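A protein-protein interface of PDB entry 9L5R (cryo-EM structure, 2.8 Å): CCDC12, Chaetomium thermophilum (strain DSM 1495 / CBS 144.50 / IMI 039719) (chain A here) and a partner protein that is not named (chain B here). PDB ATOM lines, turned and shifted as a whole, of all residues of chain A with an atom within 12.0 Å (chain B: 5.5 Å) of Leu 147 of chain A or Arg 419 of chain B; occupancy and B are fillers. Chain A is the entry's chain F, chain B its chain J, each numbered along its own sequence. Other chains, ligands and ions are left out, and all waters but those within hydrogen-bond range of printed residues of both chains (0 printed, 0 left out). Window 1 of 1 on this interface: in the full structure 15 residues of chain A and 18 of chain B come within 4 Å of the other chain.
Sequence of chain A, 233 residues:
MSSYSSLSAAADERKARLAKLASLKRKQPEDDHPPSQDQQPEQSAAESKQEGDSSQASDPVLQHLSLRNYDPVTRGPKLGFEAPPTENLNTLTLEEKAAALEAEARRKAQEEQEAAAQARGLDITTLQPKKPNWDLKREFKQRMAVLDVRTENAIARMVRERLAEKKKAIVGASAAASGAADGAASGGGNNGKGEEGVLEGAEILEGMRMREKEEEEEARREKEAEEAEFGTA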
ATOM      1  N   GLU A 139     -16.115  -4.546   2.502  1.00  0.00           N
ATOM      2  CA  GLU A 139     -14.908  -4.614   3.311  1.00  0.00           C
ATOM      3  C   GLU A 139     -13.695  -4.834   2.410  1.00  0.00           C
ATOM      4  O   GLU A 139     -12.576  -4.415   2.728  1.00  0.00           O
ATOM      5  CB  GLU A 139     -15.071  -5.717   4.363  1.00  0.00           C
ATOM      6  CG  GLU A 139     -14.019  -5.773   5.468  1.00  0.00           C
ATOM      7  CD  GLU A 139     -12.768  -6.510   5.097  1.00  0.00           C
ATOM      8  OE1 GLU A 139     -12.850  -7.419   4.255  1.00  0.00           O
ATOM      9  OE2 GLU A 139     -11.714  -6.203   5.689  1.00  0.00           O
ATOM     10  N   PHE A 140     -13.923  -5.449   1.244  1.00  0.00           N
ATOM     11  CA  PHE A 140     -12.939  -5.525   0.169  1.00  0.00           C
ATOM     12  C   PHE A 140     -12.472  -4.154  -0.309  1.00  0.00           C
ATOM     13  O   PHE A 140     -11.263  -3.880  -0.301  1.00  0.00           O
ATOM     14  CB  PHE A 140     -13.584  -6.311  -0.974  1.00  0.00           C
ATOM     15  CG  PHE A 140     -12.715  -6.530  -2.178  1.00  0.00           C
ATOM     16  CD1 PHE A 140     -11.698  -7.469  -2.179  1.00  0.00           C
ATOM     17  CD2 PHE A 140     -12.968  -5.824  -3.341  1.00  0.00           C
ATOM     18  CE1 PHE A 140     -10.947  -7.695  -3.318  1.00  0.00           C
ATOM     19  CE2 PHE A 140     -12.210  -6.025  -4.471  1.00  0.00           C
ATOM     20  CZ  PHE A 140     -11.197  -6.960  -4.463  1.00  0.00           C
ATOM     21  N   LYS A 141     -13.395  -3.272  -0.693  1.00  0.00           N
ATOM     22  CA  LYS A 141     -12.934  -1.966  -1.149  1.00  0.00           C
ATOM     23  C   LYS A 141     -12.438  -1.108   0.008  1.00  0.00           C
ATOM     24  O   LYS A 141     -11.614  -0.208  -0.195  1.00  0.00           O
ATOM     25  CB  LYS A 141     -14.021  -1.220  -1.929  1.00  0.00           C
ATOM     26  CG  LYS A 141     -15.264  -0.827  -1.162  1.00  0.00           C
ATOM     27  CD  LYS A 141     -16.239  -0.147  -2.121  1.00  0.00           C
ATOM     28  CE  LYS A 141     -17.515   0.320  -1.436  1.00  0.00           C
ATOM     29  NZ  LYS A 141     -18.360  -0.799  -0.954  1.00  0.00           N
ATOM     30  N   GLN A 142     -12.913  -1.381   1.227  1.00  0.00           N
ATOM     31  CA  GLN A 142     -12.353  -0.711   2.394  1.00  0.00           C
ATOM     32  C   GLN A 142     -10.898  -1.102   2.619  1.00  0.00           C
ATOM     33  O   GLN A 142     -10.090  -0.260   3.023  1.00  0.00           O
ATOM     34  CB  GLN A 142     -13.192  -1.028   3.630  1.00  0.00           C
ATOM     35  CG  GLN A 142     -12.766  -0.275   4.872  1.00  0.00           C
ATOM     36  CD  GLN A 142     -12.864   1.221   4.693  1.00  0.00           C
ATOM     37  OE1 GLN A 142     -11.855   1.907   4.524  1.00  0.00           O
ATOM     38  NE2 GLN A 142     -14.084   1.738   4.719  1.00  0.00           N
ATOM     39  N   ARG A 143     -10.543  -2.364   2.366  1.00  0.00           N
ATOM     40  CA  ARG A 143      -9.137  -2.737   2.444  1.00  0.00           C
ATOM     41  C   ARG A 143      -8.323  -2.159   1.301  1.00  0.00           C
ATOM     42  O   ARG A 143      -7.162  -1.789   1.505  1.00  0.00           O
ATOM     43  CB  ARG A 143      -8.962  -4.255   2.463  1.00  0.00           C
ATOM     44  CG  ARG A 143      -9.441  -4.873   3.740  1.00  0.00           C
ATOM     45  CD  ARG A 143      -9.151  -6.349   3.808  1.00  0.00           C
ATOM     46  NE  ARG A 143      -7.736  -6.600   4.039  1.00  0.00           N
ATOM     47  CZ  ARG A 143      -7.235  -7.781   4.371  1.00  0.00           C
ATOM     48  NH1 ARG A 143      -8.013  -8.836   4.541  1.00  0.00           N
ATOM     49  NH2 ARG A 143      -5.926  -7.900   4.561  1.00  0.00           N
ATOM     50  N   MET A 144      -8.887  -2.096   0.101  1.00  0.00           N
ATOM     51  CA  MET A 144      -8.289  -1.274  -0.955  1.00  0.00           C
ATOM     52  C   MET A 144      -8.932   0.098  -1.037  1.00  0.00           C
ATOM     53  O   MET A 144      -9.527   0.467  -2.044  1.00  0.00           O
ATOM     54  CB  MET A 144      -8.339  -1.979  -2.297  1.00  0.00           C
ATOM     55  CG  MET A 144      -7.291  -3.042  -2.405  1.00  0.00           C
ATOM     56  SD  MET A 144      -7.816  -4.390  -1.371  1.00  0.00           S
ATOM     57  CE  MET A 144      -9.096  -4.965  -2.435  1.00  0.00           C
ATOM     58  N   ALA A 145      -8.889   0.829   0.071  1.00  0.00           N
ATOM     59  CA  ALA A 145      -9.033   2.277   0.064  1.00  0.00           C
ATOM     60  C   ALA A 145      -7.705   2.981  -0.196  1.00  0.00           C
ATOM     61  O   ALA A 145      -7.667   4.209  -0.309  1.00  0.00           O
ATOM     62  CB  ALA A 145      -9.633   2.755   1.390  1.00  0.00           C
ATOM     63  N   VAL A 146      -6.608   2.223  -0.291  1.00  0.00           N
ATOM     64  CA  VAL A 146      -5.282   2.819  -0.447  1.00  0.00           C
ATOM     65  C   VAL A 146      -4.629   2.382  -1.757  1.00  0.00           C
ATOM     66  O   VAL A 146      -4.082   3.207  -2.506  1.00  0.00           O
ATOM     67  CB  VAL A 146      -4.395   2.469   0.763  1.00  0.00           C
ATOM     68  CG1 VAL A 146      -3.021   3.094   0.615  1.00  0.00           C
ATOM     69  CG2 VAL A 146      -5.044   2.934   2.057  1.00  0.00           C
ATOM     70  N   LEU A 147      -4.652   1.078  -2.051  1.00  0.00           N
ATOM     71  CA  LEU A 147      -3.949   0.599  -3.238  1.00  0.00           C
ATOM     72  C   LEU A 147      -4.623   1.017  -4.535  1.00  0.00           C
ATOM     73  O   LEU A 147      -3.965   1.021  -5.577  1.00  0.00           O
ATOM     74  CB  LEU A 147      -3.779  -0.919  -3.217  1.00  0.00           C
ATOM     75  CG  LEU A 147      -2.624  -1.425  -2.352  1.00  0.00           C
ATOM     76  CD1 LEU A 147      -2.408  -2.888  -2.582  1.00  0.00           C
ATOM     77  CD2 LEU A 147      -1.351  -0.683  -2.647  1.00  0.00           C
ATOM     78  N   ASP A 148      -5.902   1.389  -4.505  1.00  0.00           N
ATOM     79  CA  ASP A 148      -6.485   2.052  -5.662  1.00  0.00           C
ATOM     80  C   ASP A 148      -5.843   3.406  -5.918  1.00  0.00           C
ATOM     81  O   ASP A 148      -5.606   3.754  -7.077  1.00  0.00           O
ATOM     82  CB  ASP A 148      -7.991   2.237  -5.482  1.00  0.00           C
ATOM     83  CG  ASP A 148      -8.326   2.932  -4.195  1.00  0.00           C
ATOM     84  OD1 ASP A 148      -7.919   2.419  -3.143  1.00  0.00           O
ATOM     85  OD2 ASP A 148      -8.914   4.033  -4.243  1.00  0.00           O
ATOM     86  N   VAL A 149      -5.531   4.159  -4.859  1.00  0.00           N
ATOM     87  CA  VAL A 149      -4.799   5.412  -5.011  1.00  0.00           C
ATOM     88  C   VAL A 149      -3.392   5.147  -5.528  1.00  0.00           C
ATOM     89  O   VAL A 149      -2.894   5.882  -6.392  1.00  0.00           O
ATOM     90  CB  VAL A 149      -4.776   6.187  -3.678  1.00  0.00           C
ATOM     91  CG1 VAL A 149      -4.071   7.527  -3.839  1.00  0.00           C
ATOM     92  CG2 VAL A 149      -6.188   6.390  -3.158  1.00  0.00           C
ATOM     93  N   ARG A 150      -2.730   4.098  -5.027  1.00  0.00           N
ATOM     94  CA  ARG A 150      -1.385   3.804  -5.519  1.00  0.00           C
ATOM     95  C   ARG A 150      -1.383   3.338  -6.975  1.00  0.00           C
ATOM     96  O   ARG A 150      -0.490   3.725  -7.736  1.00  0.00           O
ATOM     97  CB  ARG A 150      -0.686   2.778  -4.629  1.00  0.00           C
ATOM     98  CG  ARG A 150       0.099   3.413  -3.485  1.00  0.00           C
ATOM     99  CD  ARG A 150       0.504   2.386  -2.449  1.00  0.00           C
ATOM    100  NE  ARG A 150       1.514   2.877  -1.520  1.00  0.00           N
ATOM    101  CZ  ARG A 150       1.788   2.313  -0.353  1.00  0.00           C
ATOM    102  NH1 ARG A 150       1.145   1.233   0.061  1.00  0.00           N
ATOM    103  NH2 ARG A 150       2.735   2.841   0.418  1.00  0.00           N
ATOM    104  N   THR A 151      -2.363   2.536  -7.398  1.00  0.00           N
ATOM    105  CA  THR A 151      -2.394   2.150  -8.807  1.00  0.00           C
ATOM    106  C   THR A 151      -2.878   3.293  -9.693  1.00  0.00           C
ATOM    107  O   THR A 151      -2.498   3.357 -10.866  1.00  0.00           O
ATOM    108  CB  THR A 151      -3.243   0.886  -9.017  1.00  0.00           C
ATOM    109  OG1 THR A 151      -3.074   0.416 -10.359  1.00  0.00           O
ATOM    110  CG2 THR A 151      -4.718   1.142  -8.784  1.00  0.00           C
ATOM    111  N   GLU A 152      -3.675   4.220  -9.152  1.00  0.00           N
ATOM    112  CA  GLU A 152      -4.012   5.443  -9.871  1.00  0.00           C
ATOM    113  C   GLU A 152      -2.770   6.294 -10.105  1.00  0.00           C
ATOM    114  O   GLU A 152      -2.564   6.819 -11.204  1.00  0.00           O
ATOM    115  CB  GLU A 152      -5.071   6.226  -9.091  1.00  0.00           C
ATOM    116  CG  GLU A 152      -5.677   7.408  -9.834  1.00  0.00           C
ATOM    117  CD  GLU A 152      -4.928   8.706  -9.589  1.00  0.00           C
ATOM    118  OE1 GLU A 152      -4.298   8.839  -8.519  1.00  0.00           O
ATOM    119  OE2 GLU A 152      -4.970   9.591 -10.468  1.00  0.00           O
ATOM    120  N   ASN A 153      -1.929   6.430  -9.081  1.00  0.00           N
ATOM    121  CA  ASN A 153      -0.655   7.115  -9.248  1.00  0.00           C
ATOM    122  C   ASN A 153       0.294   6.365 -10.172  1.00  0.00           C
ATOM    123  O   ASN A 153       1.083   7.010 -10.868  1.00  0.00           O
ATOM    124  CB  ASN A 153       0.002   7.336  -7.885  1.00  0.00           C
ATOM    125  CG  ASN A 153      -0.399   8.655  -7.257  1.00  0.00           C
ATOM    126  OD1 ASN A 153      -1.185   9.412  -7.826  1.00  0.00           O
ATOM    127  ND2 ASN A 153       0.139   8.938  -6.078  1.00  0.00           N
ATOM    128  N   ALA A 154       0.232   5.033 -10.199  1.00  0.00           N
ATOM    129  CA  ALA A 154       0.972   4.245 -11.177  1.00  0.00           C
ATOM    130  C   ALA A 154       0.531   4.527 -12.608  1.00  0.00           C
ATOM    131  O   ALA A 154       1.385   4.697 -13.485  1.00  0.00           O
ATOM    132  CB  ALA A 154       0.819   2.752 -10.879  1.00  0.00           C
ATOM    133  N   ILE A 155      -0.782   4.595 -12.852  1.00  0.00           N
ATOM    134  CA  ILE A 155      -1.290   5.012 -14.160  1.00  0.00           C
ATOM    135  C   ILE A 155      -0.844   6.433 -14.483  1.00  0.00           C
ATOM    136  O   ILE A 155      -0.471   6.733 -15.623  1.00  0.00           O
ATOM    137  CB  ILE A 155      -2.825   4.871 -14.222  1.00  0.00           C
ATOM    138  CG1 ILE A 155      -3.250   3.425 -13.978  1.00  0.00           C
ATOM    139  CG2 ILE A 155      -3.367   5.342 -15.564  1.00  0.00           C
ATOM    140  CD1 ILE A 155      -2.707   2.466 -15.010  1.00  0.00           C
ATOM    141  N   ALA A 156      -0.862   7.324 -13.487  1.00  0.00           N
ATOM    142  CA  ALA A 156      -0.469   8.714 -13.711  1.00  0.00           C
ATOM    143  C   ALA A 156       0.996   8.827 -14.124  1.00  0.00           C
ATOM    144  O   ALA A 156       1.324   9.480 -15.122  1.00  0.00           O
ATOM    145  CB  ALA A 156      -0.735   9.539 -12.451  1.00  0.00           C
ATOM    146  N   ARG A 157       1.892   8.171 -13.382  1.00  0.00           N
ATOM    147  CA  ARG A 157       3.306   8.202 -13.735  1.00  0.00           C
ATOM    148  C   ARG A 157       3.599   7.445 -15.023  1.00  0.00           C
ATOM    149  O   ARG A 157       4.516   7.832 -15.752  1.00  0.00           O
ATOM    150  CB  ARG A 157       4.164   7.664 -12.577  1.00  0.00           C
ATOM    151  CG  ARG A 157       3.969   6.197 -12.194  1.00  0.00           C
ATOM    152  CD  ARG A 157       5.014   5.274 -12.814  1.00  0.00           C
ATOM    153  NE  ARG A 157       4.687   3.867 -12.617  1.00  0.00           N
ATOM    154  CZ  ARG A 157       5.277   2.865 -13.253  1.00  0.00           C
ATOM    155  NH1 ARG A 157       6.231   3.078 -14.145  1.00  0.00           N
ATOM    156  NH2 ARG A 157       4.899   1.617 -12.991  1.00  0.00           N
ATOM    157  N   MET A 158       2.827   6.401 -15.337  1.00  0.00           N
ATOM    158  CA  MET A 158       3.014   5.689 -16.594  1.00  0.00           C
ATOM    159  C   MET A 158       2.585   6.545 -17.781  1.00  0.00           C
ATOM    160  O   MET A 158       3.245   6.533 -18.831  1.00  0.00           O
ATOM    161  CB  MET A 158       2.227   4.380 -16.536  1.00  0.00           C
ATOM    162  CG  MET A 158       2.399   3.438 -17.703  1.00  0.00           C
ATOM    163  SD  MET A 158       1.390   1.975 -17.402  1.00  0.00           S
ATOM    164  CE  MET A 158       2.316   1.194 -16.084  1.00  0.00           C
ATOM    165  N   VAL A 159       1.499   7.307 -17.619  1.00  0.00           N
ATOM    166  CA  VAL A 159       1.077   8.278 -18.626  1.00  0.00           C
ATOM    167  C   VAL A 159       2.142   9.351 -18.802  1.00  0.00           C
ATOM    168  O   VAL A 159       2.479   9.735 -19.928  1.00  0.00           O
ATOM    169  CB  VAL A 159      -0.283   8.890 -18.242  1.00  0.00           C
ATOM    170  CG1 VAL A 159      -0.551  10.183 -19.004  1.00  0.00           C
ATOM    171  CG2 VAL A 159      -1.393   7.905 -18.507  1.00  0.00           C
ATOM    172  N   GLU A 161       5.347   9.074 -18.199  1.00  0.00           N
ATOM    173  CA  GLU A 161       6.457   8.415 -18.878  1.00  0.00           C
ATOM    174  C   GLU A 161       6.224   8.296 -20.379  1.00  0.00           C
ATOM    175  O   GLU A 161       7.098   8.668 -21.172  1.00  0.00           O
ATOM    176  CB  GLU A 161       6.694   7.026 -18.282  1.00  0.00           C
ATOM    177  CG  GLU A 161       7.489   7.028 -16.990  1.00  0.00           C
ATOM    178  CD  GLU A 161       8.955   7.336 -17.213  1.00  0.00           C
ATOM    179  OE1 GLU A 161       9.486   6.959 -18.278  1.00  0.00           O
ATOM    180  OE2 GLU A 161       9.575   7.956 -16.325  1.00  0.00           O
ATOM    181  N   ILE B 376      -3.664  -9.413  -0.836  1.00  0.00           N
ATOM    182  CA  ILE B 376      -3.594  -8.061  -0.285  1.00  0.00           C
ATOM    183  C   ILE B 376      -2.685  -8.022   0.938  1.00  0.00           C
ATOM    184  O   ILE B 376      -1.964  -7.035   1.145  1.00  0.00           O
ATOM    185  CB  ILE B 376      -4.998  -7.475   0.001  1.00  0.00           C
ATOM    186  CG1 ILE B 376      -4.875  -5.987   0.264  1.00  0.00           C
ATOM    187  CG2 ILE B 376      -5.624  -8.017   1.235  1.00  0.00           C
ATOM    188  CD1 ILE B 376      -4.429  -5.263  -0.912  1.00  0.00           C
ATOM    189  N   GLU B 379       0.859  -8.058  -0.224  1.00  0.00           N
ATOM    190  CA  GLU B 379       1.259  -6.904  -1.014  1.00  0.00           C
ATOM    191  C   GLU B 379       1.406  -5.677  -0.119  1.00  0.00           C
ATOM    192  O   GLU B 379       2.311  -4.863  -0.325  1.00  0.00           O
ATOM    193  CB  GLU B 379       0.250  -6.626  -2.131  1.00  0.00           C
ATOM    194  CG  GLU B 379       0.701  -5.546  -3.108  1.00  0.00           C
ATOM    195  CD  GLU B 379      -0.327  -5.258  -4.184  1.00  0.00           C
ATOM    196  OE1 GLU B 379      -1.425  -5.848  -4.133  1.00  0.00           O
ATOM    197  OE2 GLU B 379      -0.039  -4.435  -5.081  1.00  0.00           O
ATOM    198  N   LYS B 380       0.539  -5.539   0.886  1.00  0.00           N
ATOM    199  CA  LYS B 380       0.500  -4.324   1.689  1.00  0.00           C
ATOM    200  C   LYS B 380       1.193  -4.454   3.038  1.00  0.00           C
ATOM    201  O   LYS B 380       1.607  -3.435   3.599  1.00  0.00           O
ATOM    202  CB  LYS B 380      -0.949  -3.880   1.907  1.00  0.00           C
ATOM    203  CG  LYS B 380      -1.119  -2.371   1.939  1.00  0.00           C
ATOM    204  CD  LYS B 380      -2.369  -1.959   2.697  1.00  0.00           C
ATOM    205  CE  LYS B 380      -3.631  -2.374   1.962  1.00  0.00           C
ATOM    206  NZ  LYS B 380      -4.855  -1.852   2.633  1.00  0.00           N
ATOM    207  N   ALA B 412      -7.764  -7.504  -9.872  1.00  0.00           N
ATOM    208  CA  ALA B 412      -6.845  -7.316  -8.756  1.00  0.00           C
ATOM    209  C   ALA B 412      -5.403  -7.534  -9.183  1.00  0.00           C
ATOM    210  O   ALA B 412      -4.534  -6.700  -8.909  1.00  0.00           O
ATOM    211  CB  ALA B 412      -7.218  -8.255  -7.610  1.00  0.00           C
ATOM    212  N   ALA B 414      -4.330  -7.471 -12.285  1.00  0.00           N
ATOM    213  CA  ALA B 414      -4.014  -6.472 -13.300  1.00  0.00           C
ATOM    214  C   ALA B 414      -3.507  -5.186 -12.659  1.00  0.00           C
ATOM    215  O   ALA B 414      -2.452  -4.664 -13.035  1.00  0.00           O
ATOM    216  CB  ALA B 414      -5.244  -6.199 -14.163  1.00  0.00           C
ATOM    217  N   HIS B 415      -4.231  -4.683 -11.656  1.00  0.00           N
ATOM    218  CA  HIS B 415      -3.776  -3.486 -10.954  1.00  0.00           C
ATOM    219  C   HIS B 415      -2.525  -3.750 -10.127  1.00  0.00           C
ATOM    220  O   HIS B 415      -1.711  -2.839  -9.936  1.00  0.00           O
ATOM    221  CB  HIS B 415      -4.895  -2.929 -10.080  1.00  0.00           C
ATOM    222  CG  HIS B 415      -6.063  -2.413 -10.858  1.00  0.00           C
ATOM    223  ND1 HIS B 415      -7.122  -3.211 -11.235  1.00  0.00           N
ATOM    224  CD2 HIS B 415      -6.338  -1.176 -11.331  1.00  0.00           C
ATOM    225  CE1 HIS B 415      -7.996  -2.487 -11.910  1.00  0.00           C
ATOM    226  NE2 HIS B 415      -7.546  -1.248 -11.980  1.00  0.00           N
ATOM    227  N   PHE B 416      -2.341  -4.982  -9.648  1.00  0.00           N
ATOM    228  CA  PHE B 416      -1.119  -5.324  -8.928  1.00  0.00           C
ATOM    229  C   PHE B 416       0.095  -5.250  -9.847  1.00  0.00           C
ATOM    230  O   PHE B 416       1.125  -4.668  -9.489  1.00  0.00           O
ATOM    231  CB  PHE B 416      -1.252  -6.718  -8.315  1.00  0.00           C
ATOM    232  CG  PHE B 416       0.064  -7.372  -8.002  1.00  0.00           C
ATOM    233  CD1 PHE B 416       0.839  -6.923  -6.946  1.00  0.00           C
ATOM    234  CD2 PHE B 416       0.523  -8.434  -8.762  1.00  0.00           C
ATOM    235  CE1 PHE B 416       2.048  -7.521  -6.654  1.00  0.00           C
ATOM    236  CE2 PHE B 416       1.729  -9.035  -8.473  1.00  0.00           C
ATOM    237  CZ  PHE B 416       2.493  -8.579  -7.419  1.00  0.00           C
ATOM    238  N   GLU B 417      -0.013  -5.826 -11.047  1.00  0.00           N
ATOM    239  CA  GLU B 417       1.090  -5.749 -11.997  1.00  0.00           C
ATOM    240  C   GLU B 417       1.271  -4.336 -12.533  1.00  0.00           C
ATOM    241  O   GLU B 417       2.384  -3.964 -12.918  1.00  0.00           O
ATOM    242  CB  GLU B 417       0.873  -6.732 -13.148  1.00  0.00           C
ATOM    243  CG  GLU B 417       0.853  -8.201 -12.736  1.00  0.00           C
ATOM    244  CD  GLU B 417       2.205  -8.713 -12.265  1.00  0.00           C
ATOM    245  OE1 GLU B 417       3.241  -8.112 -12.620  1.00  0.00           O
ATOM    246  OE2 GLU B 417       2.231  -9.731 -11.544  1.00  0.00           O
ATOM    247  N   ILE B 418       0.200  -3.542 -12.566  1.00  0.00           N
ATOM    248  CA  ILE B 418       0.338  -2.124 -12.887  1.00  0.00           C
ATOM    249  C   ILE B 418       1.148  -1.397 -11.816  1.00  0.00           C
ATOM    250  O   ILE B 418       2.040  -0.601 -12.142  1.00  0.00           O
ATOM    251  CB  ILE B 418      -1.053  -1.493 -13.078  1.00  0.00           C
ATOM    252  CG1 ILE B 418      -1.613  -1.855 -14.455  1.00  0.00           C
ATOM    253  CG2 ILE B 418      -1.005   0.014 -12.897  1.00  0.00           C
ATOM    254  CD1 ILE B 418      -3.097  -1.608 -14.593  1.00  0.00           C
ATOM    255  N   ARG B 419       0.865  -1.669 -10.539  1.00  0.00           N
ATOM    256  CA  ARG B 419       1.642  -1.086  -9.450  1.00  0.00           C
ATOM    257  C   ARG B 419       3.095  -1.537  -9.507  1.00  0.00           C
ATOM    258  O   ARG B 419       4.007  -0.752  -9.222  1.00  0.00           O
ATOM    259  CB  ARG B 419       1.025  -1.473  -8.106  1.00  0.00           C
ATOM    260  CG  ARG B 419      -0.123  -0.591  -7.665  1.00  0.00           C
ATOM    261  CD  ARG B 419      -0.595  -0.983  -6.279  1.00  0.00           C
ATOM    262  NE  ARG B 419      -1.242  -2.290  -6.277  1.00  0.00           N
ATOM    263  CZ  ARG B 419      -2.544  -2.485  -6.428  1.00  0.00           C
ATOM    264  NH1 ARG B 419      -3.382  -1.473  -6.582  1.00  0.00           N
ATOM    265  NH2 ARG B 419      -3.019  -3.727  -6.419  1.00  0.00           N
ATOM    266  N   GLN B 420       3.325  -2.800  -9.868  1.00  0.00           N
ATOM    267  CA  GLN B 420       4.688  -3.305 -10.003  1.00  0.00           C
ATOM    268  C   GLN B 420       5.407  -2.681 -11.193  1.00  0.00           C
ATOM    269  O   GLN B 420       6.629  -2.498 -11.155  1.00  0.00           O
ATOM    270  CB  GLN B 420       4.677  -4.829 -10.135  1.00  0.00           C
ATOM    271  CG  GLN B 420       4.178  -5.575  -8.904  1.00  0.00           C
ATOM    272  CD  GLN B 420       4.386  -4.810  -7.608  1.00  0.00           C
ATOM    273  OE1 GLN B 420       5.514  -4.650  -7.138  1.00  0.00           O
ATOM    274  NE2 GLN B 420       3.293  -4.334  -7.021  1.00  0.00           N
ATOM    275  N   GLY B 421       4.674  -2.349 -12.252  1.00  0.00           N
ATOM    276  CA  GLY B 421       5.259  -1.809 -13.459  1.00  0.00           C
ATOM    277  C   GLY B 421       5.415  -2.792 -14.600  1.00  0.00           C
ATOM    278  O   GLY B 421       6.080  -2.462 -15.588  1.00  0.00           O
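Among the printed residues, pairs that only touch across the chains: Arg 143 of chain A with Ile 376 of chain B (3.3 Å), Met 144 of chain A with Ile 376 of chain B (3.5 Å), Leu 147 of chain A with Ile 376 of chain B (3.5 Å), Leu 147 of chain A with Glu 379 of chain B (3.5 Å), Thr 151 of chain A with His 415 of chain B (3.6 Å), Thr 151 of chain A with Ile 418 of chain B (3.3 Å), Thr 151 of chain A with Arg 419 of chain B (3.4 Å), Ala 154 of chain A with Ile 418 of chain B (3.8 Å), Ile 155 of chain A with Ile 418 of chain B (3.7 Å), Arg 157 of chain A with Ile 418 of chain B (3.7 Å) and Arg 157 of chain A with Gly 421 of chain B (3.5 Å).
NH1 of Arg 419 of chain B sits at hydrogen-bond distance from O of Leu 147 of chain A, 2.8 Å away.
The side-chain amino group of Lys 380 of chain B is in hydrogen-bond range of the backbone carbonyl oxygen of Arg 143 of chain A (2.6 Å).
Printed residues of chain B within 4 Å of Met 144 of chain A: Ile 376.
Leu 147 of chain A touches just these residues of chain B: Ile 376 (3.5 Å), Glu 379 (3.5 Å) and Arg 419 (2.8 Å).
Printed residues of chain B within 4 Å of Thr 151 of chain A: His 415 (3.6 Å), Ile 418 (3.3 Å) and Arg 419 (3.4 Å).
Of the printed residues of chain B, Ala 154 of chain A touches Ile 418.
Printed residues of chain B within 4 Å of Ile 155 of chain A: Ile 418.
Printed residues of chain A within 4 Å of Ile 376 of chain B: Arg 143, Met 144 and Leu 147.
Glu 379 of chain B touches just one residue of chain A: Leu 147.
Of chain A, only Arg 143 (2.6 Å) comes within 4 Å of Lys 380 of chain B.
No residue of chain A comes within 4 Å of Ala 412 of chain B.
No residue of chain A comes within 4 Å of Phe 416 of chain B.
Of chain A, only Thr 151 (3.3 Å), Ala 154 (3.8 Å), Ile 155 (3.7 Å) and Arg 157 (3.7 Å) come within 4 Å of Ile 418 of chain B.
No residue of chain A comes within 4 Å of Gln 420 of chain B.
Of chain A, only Arg 157 (3.5 Å) comes within 4 Å of Gly 421 of chain B.
The nearest residue of chain A that does not touch Arg 419 of chain B is Arg 150 of chain A (4.1 Å).
The nearest printed residue of chain B that does not touch Ala 154 of chain A is Arg 419 of chain B (4.2 Å).
Hydrophobic or aromatic side chains of chain B that line the printed part of chain A: Ile 376, His 415 and Ile 418.
Of the 22 printed residues of chain A, 7 touch a printed residue of chain B.
Among the printed residues, 13 pairs touch across the chains.
Among the printed residues, no Asp or Glu carboxylate lies within 4 Å of a Lys or Arg side-chain nitrogen of the other chain.
The side-chain carboxylate of Glu 379 of chain B is in salt-bridge range of the guanidinium group of Arg 419 of chain B, at 2.7 Å.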
